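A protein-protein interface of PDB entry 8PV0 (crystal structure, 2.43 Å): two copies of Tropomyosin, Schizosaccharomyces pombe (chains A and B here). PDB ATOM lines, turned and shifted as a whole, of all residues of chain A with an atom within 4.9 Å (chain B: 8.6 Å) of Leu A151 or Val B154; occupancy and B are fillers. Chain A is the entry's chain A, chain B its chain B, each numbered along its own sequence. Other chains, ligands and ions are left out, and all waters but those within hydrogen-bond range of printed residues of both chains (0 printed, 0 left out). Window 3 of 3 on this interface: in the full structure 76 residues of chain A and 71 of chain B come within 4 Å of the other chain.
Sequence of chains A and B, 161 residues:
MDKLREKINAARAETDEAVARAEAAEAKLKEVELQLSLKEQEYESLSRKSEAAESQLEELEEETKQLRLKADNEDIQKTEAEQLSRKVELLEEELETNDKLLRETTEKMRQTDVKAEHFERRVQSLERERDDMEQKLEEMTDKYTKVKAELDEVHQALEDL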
ATOM      1  N   VAL A 147      -5.608 -34.445 -15.442  1.00  0.00           N
ATOM      2  CA  VAL A 147      -4.459 -33.565 -15.645  1.00  0.00           C
ATOM      3  C   VAL A 147      -3.230 -34.369 -16.050  1.00  0.00           C
ATOM      4  O   VAL A 147      -2.482 -33.969 -16.953  1.00  0.00           O
ATOM      5  CB  VAL A 147      -4.203 -32.716 -14.390  1.00  0.00           C
ATOM      6  CG1 VAL A 147      -3.006 -31.809 -14.604  1.00  0.00           C
ATOM      7  CG2 VAL A 147      -5.433 -31.892 -14.062  1.00  0.00           C
ATOM      8  N   LYS A 148      -3.000 -35.518 -15.405  1.00  0.00           N
ATOM      9  CA  LYS A 148      -1.858 -36.335 -15.791  1.00  0.00           C
ATOM     10  C   LYS A 148      -2.041 -36.924 -17.179  1.00  0.00           C
ATOM     11  O   LYS A 148      -1.056 -37.115 -17.896  1.00  0.00           O
ATOM     12  CB  LYS A 148      -1.613 -37.454 -14.777  1.00  0.00           C
ATOM     13  CG  LYS A 148      -0.339 -38.244 -15.066  1.00  0.00           C
ATOM     14  CD  LYS A 148      -0.103 -39.371 -14.074  1.00  0.00           C
ATOM     15  CE  LYS A 148       1.151 -40.151 -14.442  1.00  0.00           C
ATOM     16  NZ  LYS A 148       2.354 -39.271 -14.490  1.00  0.00           N
ATOM     17  N   ALA A 149      -3.281 -37.197 -17.588  1.00  0.00           N
ATOM     18  CA  ALA A 149      -3.512 -37.687 -18.941  1.00  0.00           C
ATOM     19  C   ALA A 149      -3.089 -36.649 -19.969  1.00  0.00           C
ATOM     20  O   ALA A 149      -2.359 -36.959 -20.920  1.00  0.00           O
ATOM     21  CB  ALA A 149      -4.984 -38.059 -19.117  1.00  0.00           C
ATOM     22  N   GLU A 150      -3.518 -35.399 -19.783  1.00  0.00           N
ATOM     23  CA  GLU A 150      -3.158 -34.389 -20.776  1.00  0.00           C
ATOM     24  C   GLU A 150      -1.671 -34.043 -20.719  1.00  0.00           C
ATOM     25  O   GLU A 150      -1.058 -33.785 -21.765  1.00  0.00           O
ATOM     26  CB  GLU A 150      -4.029 -33.143 -20.622  1.00  0.00           C
ATOM     27  CG  GLU A 150      -4.362 -32.754 -19.202  1.00  0.00           C
ATOM     28  CD  GLU A 150      -5.777 -32.227 -19.075  1.00  0.00           C
ATOM     29  OE1 GLU A 150      -6.687 -32.829 -19.685  1.00  0.00           O
ATOM     30  OE2 GLU A 150      -5.977 -31.209 -18.381  1.00  0.00           O
ATOM     31  N   LEU A 151      -1.060 -34.065 -19.530  1.00  0.00           N
ATOM     32  CA  LEU A 151       0.378 -33.824 -19.456  1.00  0.00           C
ATOM     33  C   LEU A 151       1.160 -34.952 -20.119  1.00  0.00           C
ATOM     34  O   LEU A 151       2.157 -34.703 -20.811  1.00  0.00           O
ATOM     35  CB  LEU A 151       0.812 -33.652 -18.002  1.00  0.00           C
ATOM     36  CG  LEU A 151       2.289 -33.305 -17.802  1.00  0.00           C
ATOM     37  CD1 LEU A 151       2.592 -31.939 -18.394  1.00  0.00           C
ATOM     38  CD2 LEU A 151       2.670 -33.360 -16.328  1.00  0.00           C
ATOM     39  N   ASP A 152       0.721 -36.197 -19.923  1.00  0.00           N
ATOM     40  CA  ASP A 152       1.346 -37.326 -20.599  1.00  0.00           C
ATOM     41  C   ASP A 152       1.190 -37.214 -22.105  1.00  0.00           C
ATOM     42  O   ASP A 152       2.100 -37.574 -22.855  1.00  0.00           O
ATOM     43  CB  ASP A 152       0.742 -38.638 -20.097  1.00  0.00           C
ATOM     44  CG  ASP A 152       1.181 -38.985 -18.688  1.00  0.00           C
ATOM     45  OD1 ASP A 152       1.986 -38.229 -18.104  1.00  0.00           O
ATOM     46  OD2 ASP A 152       0.717 -40.020 -18.165  1.00  0.00           O
ATOM     47  N   GLU A 153       0.043 -36.716 -22.570  1.00  0.00           N
ATOM     48  CA  GLU A 153      -0.137 -36.520 -24.005  1.00  0.00           C
ATOM     49  C   GLU A 153       0.845 -35.484 -24.542  1.00  0.00           C
ATOM     50  O   GLU A 153       1.484 -35.690 -25.585  1.00  0.00           O
ATOM     51  CB  GLU A 153      -1.577 -36.106 -24.302  1.00  0.00           C
ATOM     52  CG  GLU A 153      -1.970 -36.319 -25.750  1.00  0.00           C
ATOM     53  CD  GLU A 153      -1.913 -37.782 -26.156  1.00  0.00           C
ATOM     54  OE1 GLU A 153      -2.346 -38.642 -25.360  1.00  0.00           O
ATOM     55  OE2 GLU A 153      -1.432 -38.076 -27.271  1.00  0.00           O
ATOM     56  N   VAL A 154       0.978 -34.359 -23.834  1.00  0.00           N
ATOM     57  CA  VAL A 154       1.928 -33.324 -24.242  1.00  0.00           C
ATOM     58  C   VAL A 154       3.343 -33.893 -24.295  1.00  0.00           C
ATOM     59  O   VAL A 154       4.105 -33.627 -25.234  1.00  0.00           O
ATOM     60  CB  VAL A 154       1.838 -32.111 -23.299  1.00  0.00           C
ATOM     61  CG1 VAL A 154       2.943 -31.108 -23.604  1.00  0.00           C
ATOM     62  CG2 VAL A 154       0.474 -31.455 -23.419  1.00  0.00           C
ATOM     63  N   HIS A 155       3.710 -34.695 -23.293  1.00  0.00           N
ATOM     64  CA  HIS A 155       5.049 -35.279 -23.282  1.00  0.00           C
ATOM     65  C   HIS A 155       5.229 -36.307 -24.395  1.00  0.00           C
ATOM     66  O   HIS A 155       6.333 -36.446 -24.935  1.00  0.00           O
ATOM     67  CB  HIS A 155       5.339 -35.914 -21.920  1.00  0.00           C
ATOM     68  CG  HIS A 155       5.552 -34.921 -20.814  1.00  0.00           C
ATOM     69  ND1 HIS A 155       6.103 -33.675 -21.019  1.00  0.00           N
ATOM     70  CD2 HIS A 155       5.287 -34.999 -19.487  1.00  0.00           C
ATOM     71  CE1 HIS A 155       6.169 -33.028 -19.869  1.00  0.00           C
ATOM     72  NE2 HIS A 155       5.680 -33.809 -18.923  1.00  0.00           N
ATOM     73  N   LYS B 143      -0.633 -34.389  -5.167  1.00  0.00           N
ATOM     74  CA  LYS B 143      -0.295 -34.878  -6.502  1.00  0.00           C
ATOM     75  C   LYS B 143      -1.029 -34.088  -7.582  1.00  0.00           C
ATOM     76  O   LYS B 143      -0.440 -33.729  -8.614  1.00  0.00           O
ATOM     77  CB  LYS B 143      -0.603 -36.371  -6.608  1.00  0.00           C
ATOM     78  CG  LYS B 143       0.300 -37.242  -5.746  1.00  0.00           C
ATOM     79  CD  LYS B 143       0.291 -38.686  -6.211  1.00  0.00           C
ATOM     80  CE  LYS B 143      -1.104 -39.277  -6.157  1.00  0.00           C
ATOM     81  NZ  LYS B 143      -1.106 -40.697  -6.602  1.00  0.00           N
ATOM     82  N   LYS B 146       0.673 -30.670  -7.972  1.00  0.00           N
ATOM     83  CA  LYS B 146       1.939 -30.783  -8.690  1.00  0.00           C
ATOM     84  C   LYS B 146       1.710 -30.927 -10.191  1.00  0.00           C
ATOM     85  O   LYS B 146       2.281 -30.178 -10.997  1.00  0.00           O
ATOM     86  CB  LYS B 146       2.735 -31.968  -8.145  1.00  0.00           C
ATOM     87  CG  LYS B 146       4.126 -32.131  -8.731  1.00  0.00           C
ATOM     88  CD  LYS B 146       4.845 -33.303  -8.079  1.00  0.00           C
ATOM     89  CE  LYS B 146       6.259 -33.479  -8.617  1.00  0.00           C
ATOM     90  NZ  LYS B 146       6.962 -34.619  -7.957  1.00  0.00           N
ATOM     91  N   VAL B 147       0.859 -31.879 -10.586  1.00  0.00           N
ATOM     92  CA  VAL B 147       0.676 -32.130 -12.012  1.00  0.00           C
ATOM     93  C   VAL B 147      -0.042 -30.966 -12.687  1.00  0.00           C
ATOM     94  O   VAL B 147       0.214 -30.666 -13.860  1.00  0.00           O
ATOM     95  CB  VAL B 147      -0.057 -33.467 -12.225  1.00  0.00           C
ATOM     96  CG1 VAL B 147      -0.157 -33.793 -13.705  1.00  0.00           C
ATOM     97  CG2 VAL B 147       0.672 -34.577 -11.493  1.00  0.00           C
ATOM     98  N   LYS B 148      -0.918 -30.267 -11.960  1.00  0.00           N
ATOM     99  CA  LYS B 148      -1.617 -29.122 -12.533  1.00  0.00           C
ATOM    100  C   LYS B 148      -0.664 -27.957 -12.771  1.00  0.00           C
ATOM    101  O   LYS B 148      -0.744 -27.285 -13.807  1.00  0.00           O
ATOM    102  CB  LYS B 148      -2.764 -28.710 -11.609  1.00  0.00           C
ATOM    103  CG  LYS B 148      -3.609 -27.551 -12.108  1.00  0.00           C
ATOM    104  CD  LYS B 148      -4.299 -27.880 -13.420  1.00  0.00           C
ATOM    105  CE  LYS B 148      -5.338 -26.825 -13.769  1.00  0.00           C
ATOM    106  NZ  LYS B 148      -4.753 -25.457 -13.820  1.00  0.00           N
ATOM    107  N   ALA B 149       0.242 -27.700 -11.823  1.00  0.00           N
ATOM    108  CA  ALA B 149       1.257 -26.676 -12.043  1.00  0.00           C
ATOM    109  C   ALA B 149       2.160 -27.049 -13.212  1.00  0.00           C
ATOM    110  O   ALA B 149       2.519 -26.190 -14.028  1.00  0.00           O
ATOM    111  CB  ALA B 149       2.083 -26.462 -10.777  1.00  0.00           C
ATOM    112  N   GLU B 150       2.527 -28.329 -13.313  1.00  0.00           N
ATOM    113  CA  GLU B 150       3.331 -28.784 -14.444  1.00  0.00           C
ATOM    114  C   GLU B 150       2.619 -28.536 -15.769  1.00  0.00           C
ATOM    115  O   GLU B 150       3.223 -28.039 -16.730  1.00  0.00           O
ATOM    116  CB  GLU B 150       3.655 -30.268 -14.277  1.00  0.00           C
ATOM    117  CG  GLU B 150       5.113 -30.633 -14.479  1.00  0.00           C
ATOM    118  CD  GLU B 150       5.468 -31.960 -13.833  1.00  0.00           C
ATOM    119  OE1 GLU B 150       4.990 -32.225 -12.708  1.00  0.00           O
ATOM    120  OE2 GLU B 150       6.214 -32.746 -14.452  1.00  0.00           O
ATOM    121  N   LEU B 151       1.329 -28.878 -15.838  1.00  0.00           N
ATOM    122  CA  LEU B 151       0.567 -28.692 -17.068  1.00  0.00           C
ATOM    123  C   LEU B 151       0.419 -27.217 -17.414  1.00  0.00           C
ATOM    124  O   LEU B 151       0.506 -26.839 -18.587  1.00  0.00           O
ATOM    125  CB  LEU B 151      -0.806 -29.347 -16.937  1.00  0.00           C
ATOM    126  CG  LEU B 151      -1.675 -29.292 -18.192  1.00  0.00           C
ATOM    127  CD1 LEU B 151      -1.100 -30.195 -19.272  1.00  0.00           C
ATOM    128  CD2 LEU B 151      -3.111 -29.668 -17.873  1.00  0.00           C
ATOM    129  N   ASP B 152       0.180 -26.366 -16.414  1.00  0.00           N
ATOM    130  CA  ASP B 152       0.090 -24.934 -16.685  1.00  0.00           C
ATOM    131  C   ASP B 152       1.411 -24.393 -17.215  1.00  0.00           C
ATOM    132  O   ASP B 152       1.430 -23.588 -18.154  1.00  0.00           O
ATOM    133  CB  ASP B 152      -0.328 -24.184 -15.423  1.00  0.00           C
ATOM    134  CG  ASP B 152      -1.721 -24.553 -14.960  1.00  0.00           C
ATOM    135  OD1 ASP B 152      -2.407 -25.316 -15.675  1.00  0.00           O
ATOM    136  OD2 ASP B 152      -2.128 -24.082 -13.879  1.00  0.00           O
ATOM    137  N   GLU B 153       2.529 -24.832 -16.632  1.00  0.00           N
ATOM    138  CA  GLU B 153       3.826 -24.331 -17.075  1.00  0.00           C
ATOM    139  C   GLU B 153       4.163 -24.821 -18.478  1.00  0.00           C
ATOM    140  O   GLU B 153       4.798 -24.095 -19.253  1.00  0.00           O
ATOM    141  CB  GLU B 153       4.915 -24.738 -16.083  1.00  0.00           C
ATOM    142  CG  GLU B 153       4.769 -24.091 -14.717  1.00  0.00           C
ATOM    143  CD  GLU B 153       5.703 -24.688 -13.679  1.00  0.00           C
ATOM    144  OE1 GLU B 153       6.708 -25.317 -14.072  1.00  0.00           O
ATOM    145  OE2 GLU B 153       5.428 -24.528 -12.471  1.00  0.00           O
ATOM    146  N   VAL B 154       3.753 -26.043 -18.831  1.00  0.00           N
ATOM    147  CA  VAL B 154       4.028 -26.503 -20.192  1.00  0.00           C
ATOM    148  C   VAL B 154       3.092 -25.826 -21.191  1.00  0.00           C
ATOM    149  O   VAL B 154       3.505 -25.494 -22.311  1.00  0.00           O
ATOM    150  CB  VAL B 154       3.965 -28.043 -20.287  1.00  0.00           C
ATOM    151  CG1 VAL B 154       2.558 -28.566 -20.083  1.00  0.00           C
ATOM    152  CG2 VAL B 154       4.510 -28.512 -21.627  1.00  0.00           C
ATOM    153  N   HIS B 155       1.836 -25.580 -20.803  1.00  0.00           N
ATOM    154  CA  HIS B 155       0.916 -24.856 -21.672  1.00  0.00           C
ATOM    155  C   HIS B 155       1.395 -23.432 -21.919  1.00  0.00           C
ATOM    156  O   HIS B 155       1.232 -22.902 -23.024  1.00  0.00           O
ATOM    157  CB  HIS B 155      -0.486 -24.840 -21.057  1.00  0.00           C
ATOM    158  CG  HIS B 155      -1.325 -26.031 -21.408  1.00  0.00           C
ATOM    159  ND1 HIS B 155      -2.544 -26.276 -20.813  1.00  0.00           N
ATOM    160  CD2 HIS B 155      -1.130 -27.036 -22.296  1.00  0.00           C
ATOM    161  CE1 HIS B 155      -3.062 -27.383 -21.315  1.00  0.00           C
ATOM    162  NE2 HIS B 155      -2.224 -27.863 -22.217  1.00  0.00           N
ATOM    163  N   GLN B 156       1.977 -22.788 -20.905  1.00  0.00           N
ATOM    164  CA  GLN B 156       2.467 -21.429 -21.105  1.00  0.00           C
ATOM    165  C   GLN B 156       3.641 -21.415 -22.073  1.00  0.00           C
ATOM    166  O   GLN B 156       3.758 -20.506 -22.903  1.00  0.00           O
ATOM    167  CB  GLN B 156       2.858 -20.795 -19.769  1.00  0.00           C
ATOM    168  CG  GLN B 156       2.666 -19.275 -19.712  1.00  0.00           C
ATOM    169  CD  GLN B 156       3.804 -18.500 -20.355  1.00  0.00           C
ATOM    170  OE1 GLN B 156       4.963 -18.635 -19.960  1.00  0.00           O
ATOM    171  NE2 GLN B 156       3.477 -17.678 -21.348  1.00  0.00           N
ATOM    172  N   ALA B 157       4.512 -22.422 -21.997  1.00  0.00           N
ATOM    173  CA  ALA B 157       5.642 -22.481 -22.916  1.00  0.00           C
ATOM    174  C   ALA B 157       5.187 -22.809 -24.332  1.00  0.00           C
ATOM    175  O   ALA B 157       5.775 -22.326 -25.306  1.00  0.00           O
ATOM    176  CB  ALA B 157       6.665 -23.506 -22.430  1.00  0.00           C
ATOM    177  N   LEU B 158       4.146 -23.631 -24.469  1.00  0.00           N
ATOM    178  CA  LEU B 158       3.713 -24.014 -25.807  1.00  0.00           C
ATOM    179  C   LEU B 158       2.828 -22.951 -26.445  1.00  0.00           C
ATOM    180  O   LEU B 158       2.732 -22.896 -27.675  1.00  0.00           O
ATOM    181  CB  LEU B 158       3.010 -25.373 -25.760  1.00  0.00           C
ATOM    182  CG  LEU B 158       3.966 -26.521 -25.403  1.00  0.00           C
ATOM    183  CD1 LEU B 158       3.276 -27.876 -25.396  1.00  0.00           C
ATOM    184  CD2 LEU B 158       5.167 -26.538 -26.342  1.00  0.00           C
ATOM    185  N   GLU B 159       2.193 -22.092 -25.640  1.00  0.00           N
ATOM    186  CA  GLU B 159       1.444 -20.975 -26.203  1.00  0.00           C
ATOM    187  C   GLU B 159       2.350 -19.944 -26.861  1.00  0.00           C
ATOM    188  O   GLU B 159       1.874 -19.153 -27.681  1.00  0.00           O
ATOM    189  CB  GLU B 159       0.601 -20.294 -25.121  1.00  0.00           C
ATOM    190  CG  GLU B 159       1.294 -19.133 -24.417  1.00  0.00           C
ATOM    191  CD  GLU B 159       0.437 -18.505 -23.338  1.00  0.00           C
ATOM    192  OE1 GLU B 159      -0.701 -18.975 -23.135  1.00  0.00           O
ATOM    193  OE2 GLU B 159       0.900 -17.545 -22.689  1.00  0.00           O
ATOM    194  N   ASP B 160       3.637 -19.924 -26.511  1.00  0.00           N
ATOM    195  CA  ASP B 160       4.554 -18.959 -27.105  1.00  0.00           C
ATOM    196  C   ASP B 160       4.890 -19.339 -28.544  1.00  0.00           C
ATOM    197  O   ASP B 160       4.702 -18.543 -29.470  1.00  0.00           O
ATOM    198  CB  ASP B 160       5.824 -18.851 -26.256  1.00  0.00           C
ATOM    199  CG  ASP B 160       5.623 -18.014 -25.007  1.00  0.00           C
ATOM    200  OD1 ASP B 160       5.037 -16.914 -25.107  1.00  0.00           O
ATOM    201  OD2 ASP B 160       6.058 -18.460 -23.927  1.00  0.00           O
ATOM    202  N   LEU B 161       5.392 -20.554 -28.748  1.00  0.00           N
ATOM    203  CA  LEU B 161       5.745 -21.025 -30.085  1.00  0.00           C
ATOM    204  C   LEU B 161       5.440 -22.512 -30.249  1.00  0.00           C
ATOM    205  O   LEU B 161       5.526 -23.060 -31.347  1.00  0.00           O
ATOM    206  CB  LEU B 161       7.223 -20.764 -30.372  1.00  0.00           C
ATOM    207  CG  LEU B 161       7.617 -19.332 -30.736  1.00  0.00           C
ATOM    208  CD1 LEU B 161       9.126 -19.208 -30.887  1.00  0.00           C
ATOM    209  CD2 LEU B 161       6.914 -18.899 -32.011  1.00  0.00           C
ATOM    210  OXT LEU B 161       5.113 -23.206 -29.288  1.00  0.00           O
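NZ of Lys A148 is in salt-bridge range of OD1 of Asp A152 (3.8 Å). The side-chain amino group (NZ) of Lys B148 is in salt-bridge range of the side-chain carboxylate (OD2) of Asp B152, 3.0 Å away.
Val A147 touches Val B147 (CG1 to O, 3.5 Å). CA of Lys B148 touches CG1 of Val A147 (3.7 Å). Lys A148 touches Val B147 (CA to CG1, 3.7 Å). Glu A150 touches Leu B151 (OE2 to CD2, 3.3 Å). Leu A151 touches Val B147 (CD2 to CG1, 3.9 Å). CB of Glu B150 touches CD2 of Leu A151 (3.8 Å). CD1 of Leu B151 touches N of Leu A151, 3.9 Å away. CD1 of Leu A151 touches CG1 of Val B154, 3.8 Å away. CG1 of Val A154 touches CG2 of Val B154, 3.6 Å away. Val A154 touches Leu B158.
Of chain B, only Val B147 (3.9 Å), Glu B150 (3.8 Å), Leu B151 (3.9 Å) and Val B154 (3.8 Å) come within 4 Å of Leu A151. Val B154 touches two residues of chain A. Of the printed residues of chain B, Val A147 touches Val B147 (3.5 Å), Lys B148 (3.7 Å) and Leu B151 (3.9 Å). Printed residues of chain B within 4 Å of Val A154: Val B154 and Leu B158.
Printed residues of chain A that touch a printed residue of chain B: Val A147, Lys A148, Glu A150, Leu A151 and Val A154. Hydrophobic or aromatic side chains of chain A within 4 Å of the printed part of chain B: Val A147, Leu A151 and Val A154. Of the 17 printed residues of chain B, 6 touch a printed residue of chain A. Printed residues of chain B that touch a printed residue of chain A: Val B147, Lys B148, Glu B150, Leu B151, Val B154 and Leu B158. Among the printed residues, 11 pairs touch across the chains.
Val A147 touches Leu B151, and with the chains exchanged Leu A151 touches Val B147. Leu B151 touches its own counterpart, Leu A151. Leu A151 touches Val B154, but with the chains exchanged Val A154 does not touch Leu B151 (4.6 Å). Val A154 touches its own counterpart, Val B154. Positions printed for both chains: 147, 148, 149, 150, 151, 152, 153, 154 and 155.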
